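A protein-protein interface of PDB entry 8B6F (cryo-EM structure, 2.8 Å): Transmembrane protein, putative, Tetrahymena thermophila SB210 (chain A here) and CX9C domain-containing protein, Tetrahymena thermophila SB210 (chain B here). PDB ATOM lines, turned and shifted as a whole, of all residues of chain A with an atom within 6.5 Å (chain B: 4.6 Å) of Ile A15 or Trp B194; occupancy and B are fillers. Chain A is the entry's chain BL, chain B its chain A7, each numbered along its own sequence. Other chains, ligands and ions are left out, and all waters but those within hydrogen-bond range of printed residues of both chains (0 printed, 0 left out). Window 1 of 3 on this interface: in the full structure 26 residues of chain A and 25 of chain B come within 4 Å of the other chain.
ND2 of Asn B230 lies within hydrogen-bond range of O of Gly A14.
OD2 of Asp A133 lies within hydrogen-bond range of NE2 of Gln B197.
The side-chain amide nitrogen (ND2) of Asn A131 lies close to the side-chain amide nitrogen (ND2) of Asn B196.
NE2 of Gln B197 lies close to NH2 of Arg A135 (3.2 Å).
NE1 of Trp B194 lies close to SG of Cys B180 (3.7 Å).
The side-chain sulfur (SG) of Cys B191 forms a disulfide with the side-chain sulfur (SG) of Cys B180, 2.0 Å away.
The side-chain carboxylate (OD2) of Asp B176 is in salt-bridge range of the side-chain amino group (NZ) of Lys B223 (3.4 Å).
The side-chain carboxylate (OD2) of Asp A133 is in salt-bridge range of the guanidinium group (NH2) of Arg A135 (2.5 Å).
Among the printed residues, merely in contact across the chains: Asp A12 with Asn B230 (3.9 Å), Ile A15 with Trp B194 (3.8 Å), Ile A15 with Lys B223 (3.7 Å), Ile A15 with Lys B224 (3.3 Å), Ile A15 with Phe B225 (3.6 Å), Val A16 with Asn B230 (3.8 Å) and Asn A131 with Thr B193 (3.6 Å).
Ile A15 touches just these residues of chain B: Trp B194, Lys B223, Lys B224 and Phe B225.
Of chain A, only Ile A15 comes within 4 Å of Trp B194.
Printed residues of chain B within 4 Å of Asn A131: Thr B193 (3.6 Å) and Asn B196 (3.3 Å).
Of the printed residues of chain A, Lys B224 touches Ile A15.
Printed residues of chain B within 4 Å of Arg A135: Gln B197 (3.2 Å).
Printed residues of chain A within 4 Å of Lys B223: Ile A15.
Of the printed residues of chain A, Asn B196 touches Asn A131 (3.3 Å).
The nearest residue of chain B that does not touch Ile A15 is Asn B230 (4.1 Å).
The nearest residue of chain A that does not touch Trp B194 is Asp A133 (5.5 Å).
Hydrophobic or aromatic side chains of chain A that line the printed part of chain B: Ile A15.
Of the 17 printed residues of chain B, 8 touch a printed residue of chain A.
Printed residues of chain B that touch a printed residue of chain A: Thr B193, Trp B194, Asn B196, Gln B197, Lys B223, Lys B224, Phe B225 and Asn B230.
Among the printed residues, 11 pairs touch across the chains.
Among the printed residues, no Asp or Glu carboxylate lies within 4 Å of a Lys or Arg side-chain nitrogen of the other chain.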
ATOM      1  N   THR A  11     -16.979  33.931  10.898  1.00  0.00           N
ATOM      2  CA  THR A  11     -16.305  32.640  10.876  1.00  0.00           C
ATOM      3  C   THR A  11     -14.961  32.710  11.590  1.00  0.00           C
ATOM      4  O   THR A  11     -14.209  33.677  11.447  1.00  0.00           O
ATOM      5  CB  THR A  11     -16.106  32.172   9.433  1.00  0.00           C
ATOM      6  OG1 THR A  11     -17.382  31.933   8.824  1.00  0.00           O
ATOM      7  CG2 THR A  11     -15.284  30.889   9.377  1.00  0.00           C
ATOM      8  N   ASP A  12     -14.659  31.660  12.357  1.00  0.00           N
ATOM      9  CA  ASP A  12     -13.386  31.540  13.068  1.00  0.00           C
ATOM     10  C   ASP A  12     -13.135  32.747  13.967  1.00  0.00           C
ATOM     11  O   ASP A  12     -12.006  33.225  14.094  1.00  0.00           O
ATOM     12  CB  ASP A  12     -12.227  31.347  12.090  1.00  0.00           C
ATOM     13  CG  ASP A  12     -12.321  30.043  11.325  1.00  0.00           C
ATOM     14  OD1 ASP A  12     -12.901  29.077  11.864  1.00  0.00           O
ATOM     15  OD2 ASP A  12     -11.814  29.981  10.185  1.00  0.00           O
ATOM     16  N   SER A  13     -14.191  33.237  14.605  1.00  0.00           N
ATOM     17  CA  SER A  13     -14.099  34.351  15.538  1.00  0.00           C
ATOM     18  C   SER A  13     -14.207  33.802  16.954  1.00  0.00           C
ATOM     19  O   SER A  13     -15.196  33.144  17.294  1.00  0.00           O
ATOM     20  CB  SER A  13     -15.198  35.379  15.270  1.00  0.00           C
ATOM     21  OG  SER A  13     -15.043  36.519  16.095  1.00  0.00           O
ATOM     22  N   GLY A  14     -13.197  34.074  17.774  1.00  0.00           N
ATOM     23  CA  GLY A  14     -13.154  33.499  19.100  1.00  0.00           C
ATOM     24  C   GLY A  14     -12.479  32.145  19.086  1.00  0.00           C
ATOM     25  O   GLY A  14     -11.249  32.053  19.126  1.00  0.00           O
ATOM     26  N   ILE A  15     -13.278  31.086  19.034  1.00  0.00           N
ATOM     27  CA  ILE A  15     -12.784  29.718  18.941  1.00  0.00           C
ATOM     28  C   ILE A  15     -12.801  29.293  17.480  1.00  0.00           C
ATOM     29  O   ILE A  15     -13.750  29.593  16.745  1.00  0.00           O
ATOM     30  CB  ILE A  15     -13.629  28.764  19.808  1.00  0.00           C
ATOM     31  CG1 ILE A  15     -12.970  27.383  19.865  1.00  0.00           C
ATOM     32  CG2 ILE A  15     -15.054  28.665  19.269  1.00  0.00           C
ATOM     33  CD1 ILE A  15     -13.677  26.393  20.769  1.00  0.00           C
ATOM     34  N   VAL A  16     -11.747  28.607  17.053  1.00  0.00           N
ATOM     35  CA  VAL A  16     -11.654  28.091  15.692  1.00  0.00           C
ATOM     36  C   VAL A  16     -12.153  26.652  15.686  1.00  0.00           C
ATOM     37  O   VAL A  16     -11.681  25.816  16.464  1.00  0.00           O
ATOM     38  CB  VAL A  16     -10.213  28.191  15.160  1.00  0.00           C
ATOM     39  CG1 VAL A  16      -9.263  27.287  15.945  1.00  0.00           C
ATOM     40  CG2 VAL A  16     -10.172  27.849  13.680  1.00  0.00           C
ATOM     41  N   ILE A  17     -13.124  26.368  14.823  1.00  0.00           N
ATOM     42  CA  ILE A  17     -13.784  25.069  14.773  1.00  0.00           C
ATOM     43  C   ILE A  17     -13.546  24.455  13.403  1.00  0.00           C
ATOM     44  O   ILE A  17     -13.814  25.088  12.375  1.00  0.00           O
ATOM     45  CB  ILE A  17     -15.291  25.189  15.072  1.00  0.00           C
ATOM     46  CG1 ILE A  17     -15.983  23.825  14.983  1.00  0.00           C
ATOM     47  CG2 ILE A  17     -15.960  26.177  14.125  1.00  0.00           C
ATOM     48  CD1 ILE A  17     -15.417  22.778  15.917  1.00  0.00           C
ATOM     49  N   ASN A 131     -26.311  29.351  11.352  1.00  0.00           N
ATOM     50  CA  ASN A 131     -25.301  28.887  12.288  1.00  0.00           C
ATOM     51  C   ASN A 131     -24.409  27.843  11.626  1.00  0.00           C
ATOM     52  O   ASN A 131     -24.729  27.291  10.573  1.00  0.00           O
ATOM     53  CB  ASN A 131     -25.959  28.298  13.535  1.00  0.00           C
ATOM     54  CG  ASN A 131     -26.931  29.259  14.185  1.00  0.00           C
ATOM     55  OD1 ASN A 131     -26.549  30.086  15.010  1.00  0.00           O
ATOM     56  ND2 ASN A 131     -28.203  29.149  13.819  1.00  0.00           N
ATOM     57  N   ASP A 133     -23.727  24.930  12.895  1.00  0.00           N
ATOM     58  CA  ASP A 133     -24.106  23.588  13.311  1.00  0.00           C
ATOM     59  C   ASP A 133     -25.194  23.028  12.409  1.00  0.00           C
ATOM     60  O   ASP A 133     -26.117  23.743  12.009  1.00  0.00           O
ATOM     61  CB  ASP A 133     -24.593  23.591  14.761  1.00  0.00           C
ATOM     62  CG  ASP A 133     -23.509  23.993  15.738  1.00  0.00           C
ATOM     63  OD1 ASP A 133     -22.348  24.163  15.307  1.00  0.00           O
ATOM     64  OD2 ASP A 133     -23.816  24.141  16.940  1.00  0.00           O
ATOM     65  N   ARG A 135     -26.951  20.515  13.617  1.00  0.00           N
ATOM     66  CA  ARG A 135     -27.860  19.897  14.572  1.00  0.00           C
ATOM     67  C   ARG A 135     -29.274  20.449  14.472  1.00  0.00           C
ATOM     68  O   ARG A 135     -30.209  19.811  14.964  1.00  0.00           O
ATOM     69  CB  ARG A 135     -27.330  20.088  15.992  1.00  0.00           C
ATOM     70  CG  ARG A 135     -26.140  19.206  16.314  1.00  0.00           C
ATOM     71  CD  ARG A 135     -25.573  19.485  17.696  1.00  0.00           C
ATOM     72  NE  ARG A 135     -24.905  20.779  17.767  1.00  0.00           N
ATOM     73  CZ  ARG A 135     -24.201  21.203  18.807  1.00  0.00           C
ATOM     74  NH1 ARG A 135     -24.040  20.455  19.886  1.00  0.00           N
ATOM     75  NH2 ARG A 135     -23.640  22.408  18.762  1.00  0.00           N
ATOM     76  N   SER B 173     -25.263  25.466  27.391  1.00  0.00           N
ATOM     77  CA  SER B 173     -25.316  26.503  26.368  1.00  0.00           C
ATOM     78  C   SER B 173     -25.185  27.887  26.989  1.00  0.00           C
ATOM     79  O   SER B 173     -24.500  28.759  26.444  1.00  0.00           O
ATOM     80  CB  SER B 173     -26.617  26.397  25.575  1.00  0.00           C
ATOM     81  OG  SER B 173     -26.748  25.115  24.986  1.00  0.00           O
ATOM     82  N   ASP B 176     -21.461  28.441  27.944  1.00  0.00           N
ATOM     83  CA  ASP B 176     -20.573  28.707  26.818  1.00  0.00           C
ATOM     84  C   ASP B 176     -20.840  30.087  26.233  1.00  0.00           C
ATOM     85  O   ASP B 176     -19.908  30.779  25.810  1.00  0.00           O
ATOM     86  CB  ASP B 176     -20.703  27.607  25.758  1.00  0.00           C
ATOM     87  CG  ASP B 176     -22.031  27.634  25.020  1.00  0.00           C
ATOM     88  OD1 ASP B 176     -22.630  28.716  24.860  1.00  0.00           O
ATOM     89  OD2 ASP B 176     -22.475  26.551  24.583  1.00  0.00           O
ATOM     90  N   SER B 177     -22.108  30.498  26.189  1.00  0.00           N
ATOM     91  CA  SER B 177     -22.428  31.849  25.745  1.00  0.00           C
ATOM     92  C   SER B 177     -21.828  32.884  26.688  1.00  0.00           C
ATOM     93  O   SER B 177     -21.322  33.921  26.243  1.00  0.00           O
ATOM     94  CB  SER B 177     -23.943  32.020  25.651  1.00  0.00           C
ATOM     95  OG  SER B 177     -24.279  33.313  25.186  1.00  0.00           O
ATOM     96  N   CYS B 180     -18.139  33.105  25.959  1.00  0.00           N
ATOM     97  CA  CYS B 180     -17.899  33.850  24.729  1.00  0.00           C
ATOM     98  C   CYS B 180     -18.057  35.345  24.963  1.00  0.00           C
ATOM     99  O   CYS B 180     -17.232  36.148  24.516  1.00  0.00           O
ATOM    100  CB  CYS B 180     -18.852  33.369  23.635  1.00  0.00           C
ATOM    101  SG  CYS B 180     -18.512  34.061  22.001  1.00  0.00           S
ATOM    102  N   CYS B 191     -20.785  36.252  19.226  1.00  0.00           N
ATOM    103  CA  CYS B 191     -21.281  35.161  20.055  1.00  0.00           C
ATOM    104  C   CYS B 191     -22.736  34.816  19.769  1.00  0.00           C
ATOM    105  O   CYS B 191     -23.349  34.081  20.548  1.00  0.00           O
ATOM    106  CB  CYS B 191     -21.118  35.512  21.534  1.00  0.00           C
ATOM    107  SG  CYS B 191     -19.422  35.875  22.016  1.00  0.00           S
ATOM    108  N   LYS B 192     -23.309  35.328  18.677  1.00  0.00           N
ATOM    109  CA  LYS B 192     -24.718  35.069  18.410  1.00  0.00           C
ATOM    110  C   LYS B 192     -24.991  33.587  18.200  1.00  0.00           C
ATOM    111  O   LYS B 192     -26.089  33.111  18.508  1.00  0.00           O
ATOM    112  CB  LYS B 192     -25.184  35.870  17.194  1.00  0.00           C
ATOM    113  CG  LYS B 192     -24.648  35.377  15.862  1.00  0.00           C
ATOM    114  CD  LYS B 192     -25.242  36.183  14.721  1.00  0.00           C
ATOM    115  CE  LYS B 192     -24.954  35.534  13.382  1.00  0.00           C
ATOM    116  NZ  LYS B 192     -25.637  36.251  12.270  1.00  0.00           N
ATOM    117  N   THR B 193     -24.019  32.842  17.674  1.00  0.00           N
ATOM    118  CA  THR B 193     -24.223  31.412  17.461  1.00  0.00           C
ATOM    119  C   THR B 193     -24.491  30.698  18.778  1.00  0.00           C
ATOM    120  O   THR B 193     -25.398  29.864  18.874  1.00  0.00           O
ATOM    121  CB  THR B 193     -23.010  30.803  16.757  1.00  0.00           C
ATOM    122  OG1 THR B 193     -21.823  31.090  17.507  1.00  0.00           O
ATOM    123  CG2 THR B 193     -22.872  31.362  15.351  1.00  0.00           C
ATOM    124  N   TRP B 194     -23.703  31.009  19.807  1.00  0.00           N
ATOM    125  CA  TRP B 194     -23.920  30.393  21.111  1.00  0.00           C
ATOM    126  C   TRP B 194     -25.187  30.927  21.764  1.00  0.00           C
ATOM    127  O   TRP B 194     -25.936  30.171  22.391  1.00  0.00           O
ATOM    128  CB  TRP B 194     -22.709  30.628  22.010  1.00  0.00           C
ATOM    129  CG  TRP B 194     -21.413  30.458  21.294  1.00  0.00           C
ATOM    130  CD1 TRP B 194     -20.542  31.442  20.938  1.00  0.00           C
ATOM    131  CD2 TRP B 194     -20.847  29.229  20.826  1.00  0.00           C
ATOM    132  NE1 TRP B 194     -19.462  30.902  20.284  1.00  0.00           N
ATOM    133  CE2 TRP B 194     -19.625  29.544  20.205  1.00  0.00           C
ATOM    134  CE3 TRP B 194     -21.253  27.892  20.880  1.00  0.00           C
ATOM    135  CZ2 TRP B 194     -18.805  28.573  19.637  1.00  0.00           C
ATOM    136  CZ3 TRP B 194     -20.437  26.928  20.315  1.00  0.00           C
ATOM    137  CH2 TRP B 194     -19.226  27.273  19.702  1.00  0.00           C
ATOM    138  N   ILE B 195     -25.440  32.229  21.630  1.00  0.00           N
ATOM    139  CA  ILE B 195     -26.693  32.794  22.117  1.00  0.00           C
ATOM    140  C   ILE B 195     -27.870  32.186  21.369  1.00  0.00           C
ATOM    141  O   ILE B 195     -28.926  31.920  21.952  1.00  0.00           O
ATOM    142  CB  ILE B 195     -26.675  34.329  21.990  1.00  0.00           C
ATOM    143  CG1 ILE B 195     -25.559  34.918  22.857  1.00  0.00           C
ATOM    144  CG2 ILE B 195     -28.027  34.912  22.381  1.00  0.00           C
ATOM    145  CD1 ILE B 195     -25.336  36.403  22.660  1.00  0.00           C
ATOM    146  N   ASN B 196     -27.698  31.931  20.072  1.00  0.00           N
ATOM    147  CA  ASN B 196     -28.755  31.287  19.301  1.00  0.00           C
ATOM    148  C   ASN B 196     -29.003  29.868  19.796  1.00  0.00           C
ATOM    149  O   ASN B 196     -30.155  29.425  19.870  1.00  0.00           O
ATOM    150  CB  ASN B 196     -28.396  31.292  17.816  1.00  0.00           C
ATOM    151  CG  ASN B 196     -29.585  30.982  16.928  1.00  0.00           C
ATOM    152  OD1 ASN B 196     -30.516  30.288  17.334  1.00  0.00           O
ATOM    153  ND2 ASN B 196     -29.559  31.499  15.706  1.00  0.00           N
ATOM    154  N   GLN B 197     -27.941  29.136  20.136  1.00  0.00           N
ATOM    155  CA  GLN B 197     -28.127  27.812  20.716  1.00  0.00           C
ATOM    156  C   GLN B 197     -28.891  27.898  22.030  1.00  0.00           C
ATOM    157  O   GLN B 197     -29.775  27.077  22.299  1.00  0.00           O
ATOM    158  CB  GLN B 197     -26.777  27.132  20.938  1.00  0.00           C
ATOM    159  CG  GLN B 197     -26.095  26.669  19.666  1.00  0.00           C
ATOM    160  CD  GLN B 197     -24.884  25.806  19.947  1.00  0.00           C
ATOM    161  OE1 GLN B 197     -24.674  25.361  21.074  1.00  0.00           O
ATOM    162  NE2 GLN B 197     -24.077  25.566  18.919  1.00  0.00           N
ATOM    163  N   TYR B 198     -28.559  28.883  22.866  1.00  0.00           N
ATOM    164  CA  TYR B 198     -29.273  29.054  24.127  1.00  0.00           C
ATOM    165  C   TYR B 198     -30.744  29.373  23.885  1.00  0.00           C
ATOM    166  O   TYR B 198     -31.621  28.863  24.590  1.00  0.00           O
ATOM    167  CB  TYR B 198     -28.613  30.151  24.959  1.00  0.00           C
ATOM    168  CG  TYR B 198     -29.366  30.476  26.224  1.00  0.00           C
ATOM    169  CD1 TYR B 198     -29.284  29.646  27.334  1.00  0.00           C
ATOM    170  CD2 TYR B 198     -30.156  31.612  26.310  1.00  0.00           C
ATOM    171  CE1 TYR B 198     -29.970  29.939  28.492  1.00  0.00           C
ATOM    172  CE2 TYR B 198     -30.848  31.913  27.463  1.00  0.00           C
ATOM    173  CZ  TYR B 198     -30.750  31.072  28.551  1.00  0.00           C
ATOM    174  OH  TYR B 198     -31.438  31.370  29.701  1.00  0.00           O
ATOM    175  N   SER B 222     -14.435  20.897  25.000  1.00  0.00           N
ATOM    176  CA  SER B 222     -14.382  22.156  25.726  1.00  0.00           C
ATOM    177  C   SER B 222     -14.230  23.319  24.753  1.00  0.00           C
ATOM    178  O   SER B 222     -13.417  23.267  23.826  1.00  0.00           O
ATOM    179  CB  SER B 222     -13.218  22.134  26.715  1.00  0.00           C
ATOM    180  OG  SER B 222     -13.097  23.371  27.391  1.00  0.00           O
ATOM    181  N   LYS B 223     -15.014  24.371  24.972  1.00  0.00           N
ATOM    182  CA  LYS B 223     -15.038  25.536  24.095  1.00  0.00           C
ATOM    183  C   LYS B 223     -14.271  26.671  24.764  1.00  0.00           C
ATOM    184  O   LYS B 223     -14.764  27.287  25.713  1.00  0.00           O
ATOM    185  CB  LYS B 223     -16.477  25.947  23.787  1.00  0.00           C
ATOM    186  CG  LYS B 223     -17.275  24.871  23.067  1.00  0.00           C
ATOM    187  CD  LYS B 223     -18.754  25.212  23.011  1.00  0.00           C
ATOM    188  CE  LYS B 223     -19.546  24.110  22.324  1.00  0.00           C
ATOM    189  NZ  LYS B 223     -21.018  24.338  22.413  1.00  0.00           N
ATOM    190  N   LYS B 224     -13.070  26.944  24.265  1.00  0.00           N
ATOM    191  CA  LYS B 224     -12.221  28.012  24.771  1.00  0.00           C
ATOM    192  C   LYS B 224     -12.133  29.113  23.724  1.00  0.00           C
ATOM    193  O   LYS B 224     -11.860  28.836  22.552  1.00  0.00           O
ATOM    194  CB  LYS B 224     -10.824  27.488  25.108  1.00  0.00           C
ATOM    195  CG  LYS B 224     -10.823  26.346  26.110  1.00  0.00           C
ATOM    196  CD  LYS B 224      -9.415  25.828  26.350  1.00  0.00           C
ATOM    197  CE  LYS B 224      -9.406  24.685  27.348  1.00  0.00           C
ATOM    198  NZ  LYS B 224      -9.947  25.096  28.673  1.00  0.00           N
ATOM    199  N   PHE B 225     -12.359  30.352  24.148  1.00  0.00           N
ATOM    200  CA  PHE B 225     -12.379  31.500  23.252  1.00  0.00           C
ATOM    201  C   PHE B 225     -11.173  32.386  23.530  1.00  0.00           C
ATOM    202  O   PHE B 225     -10.907  32.736  24.683  1.00  0.00           O
ATOM    203  CB  PHE B 225     -13.673  32.301  23.415  1.00  0.00           C
ATOM    204  CG  PHE B 225     -14.917  31.496  23.183  1.00  0.00           C
ATOM    205  CD1 PHE B 225     -15.468  30.742  24.204  1.00  0.00           C
ATOM    206  CD2 PHE B 225     -15.539  31.501  21.948  1.00  0.00           C
ATOM    207  CE1 PHE B 225     -16.615  30.001  23.995  1.00  0.00           C
ATOM    208  CE2 PHE B 225     -16.685  30.764  21.732  1.00  0.00           C
ATOM    209  CZ  PHE B 225     -17.224  30.013  22.757  1.00  0.00           C
ATOM    210  N   ASN B 230      -7.478  34.393  17.685  1.00  0.00           N
ATOM    211  CA  ASN B 230      -8.400  34.177  16.571  1.00  0.00           C
ATOM    212  C   ASN B 230      -9.289  35.410  16.443  1.00  0.00           C
ATOM    213  O   ASN B 230     -10.401  35.450  16.974  1.00  0.00           O
ATOM    214  CB  ASN B 230      -9.221  32.915  16.798  1.00  0.00           C
ATOM    215  CG  ASN B 230      -8.374  31.743  17.245  1.00  0.00           C
ATOM    216  OD1 ASN B 230      -7.238  31.583  16.807  1.00  0.00           O
ATOM    217  ND2 ASN B 230      -8.927  30.915  18.123  1.00  0.00           N
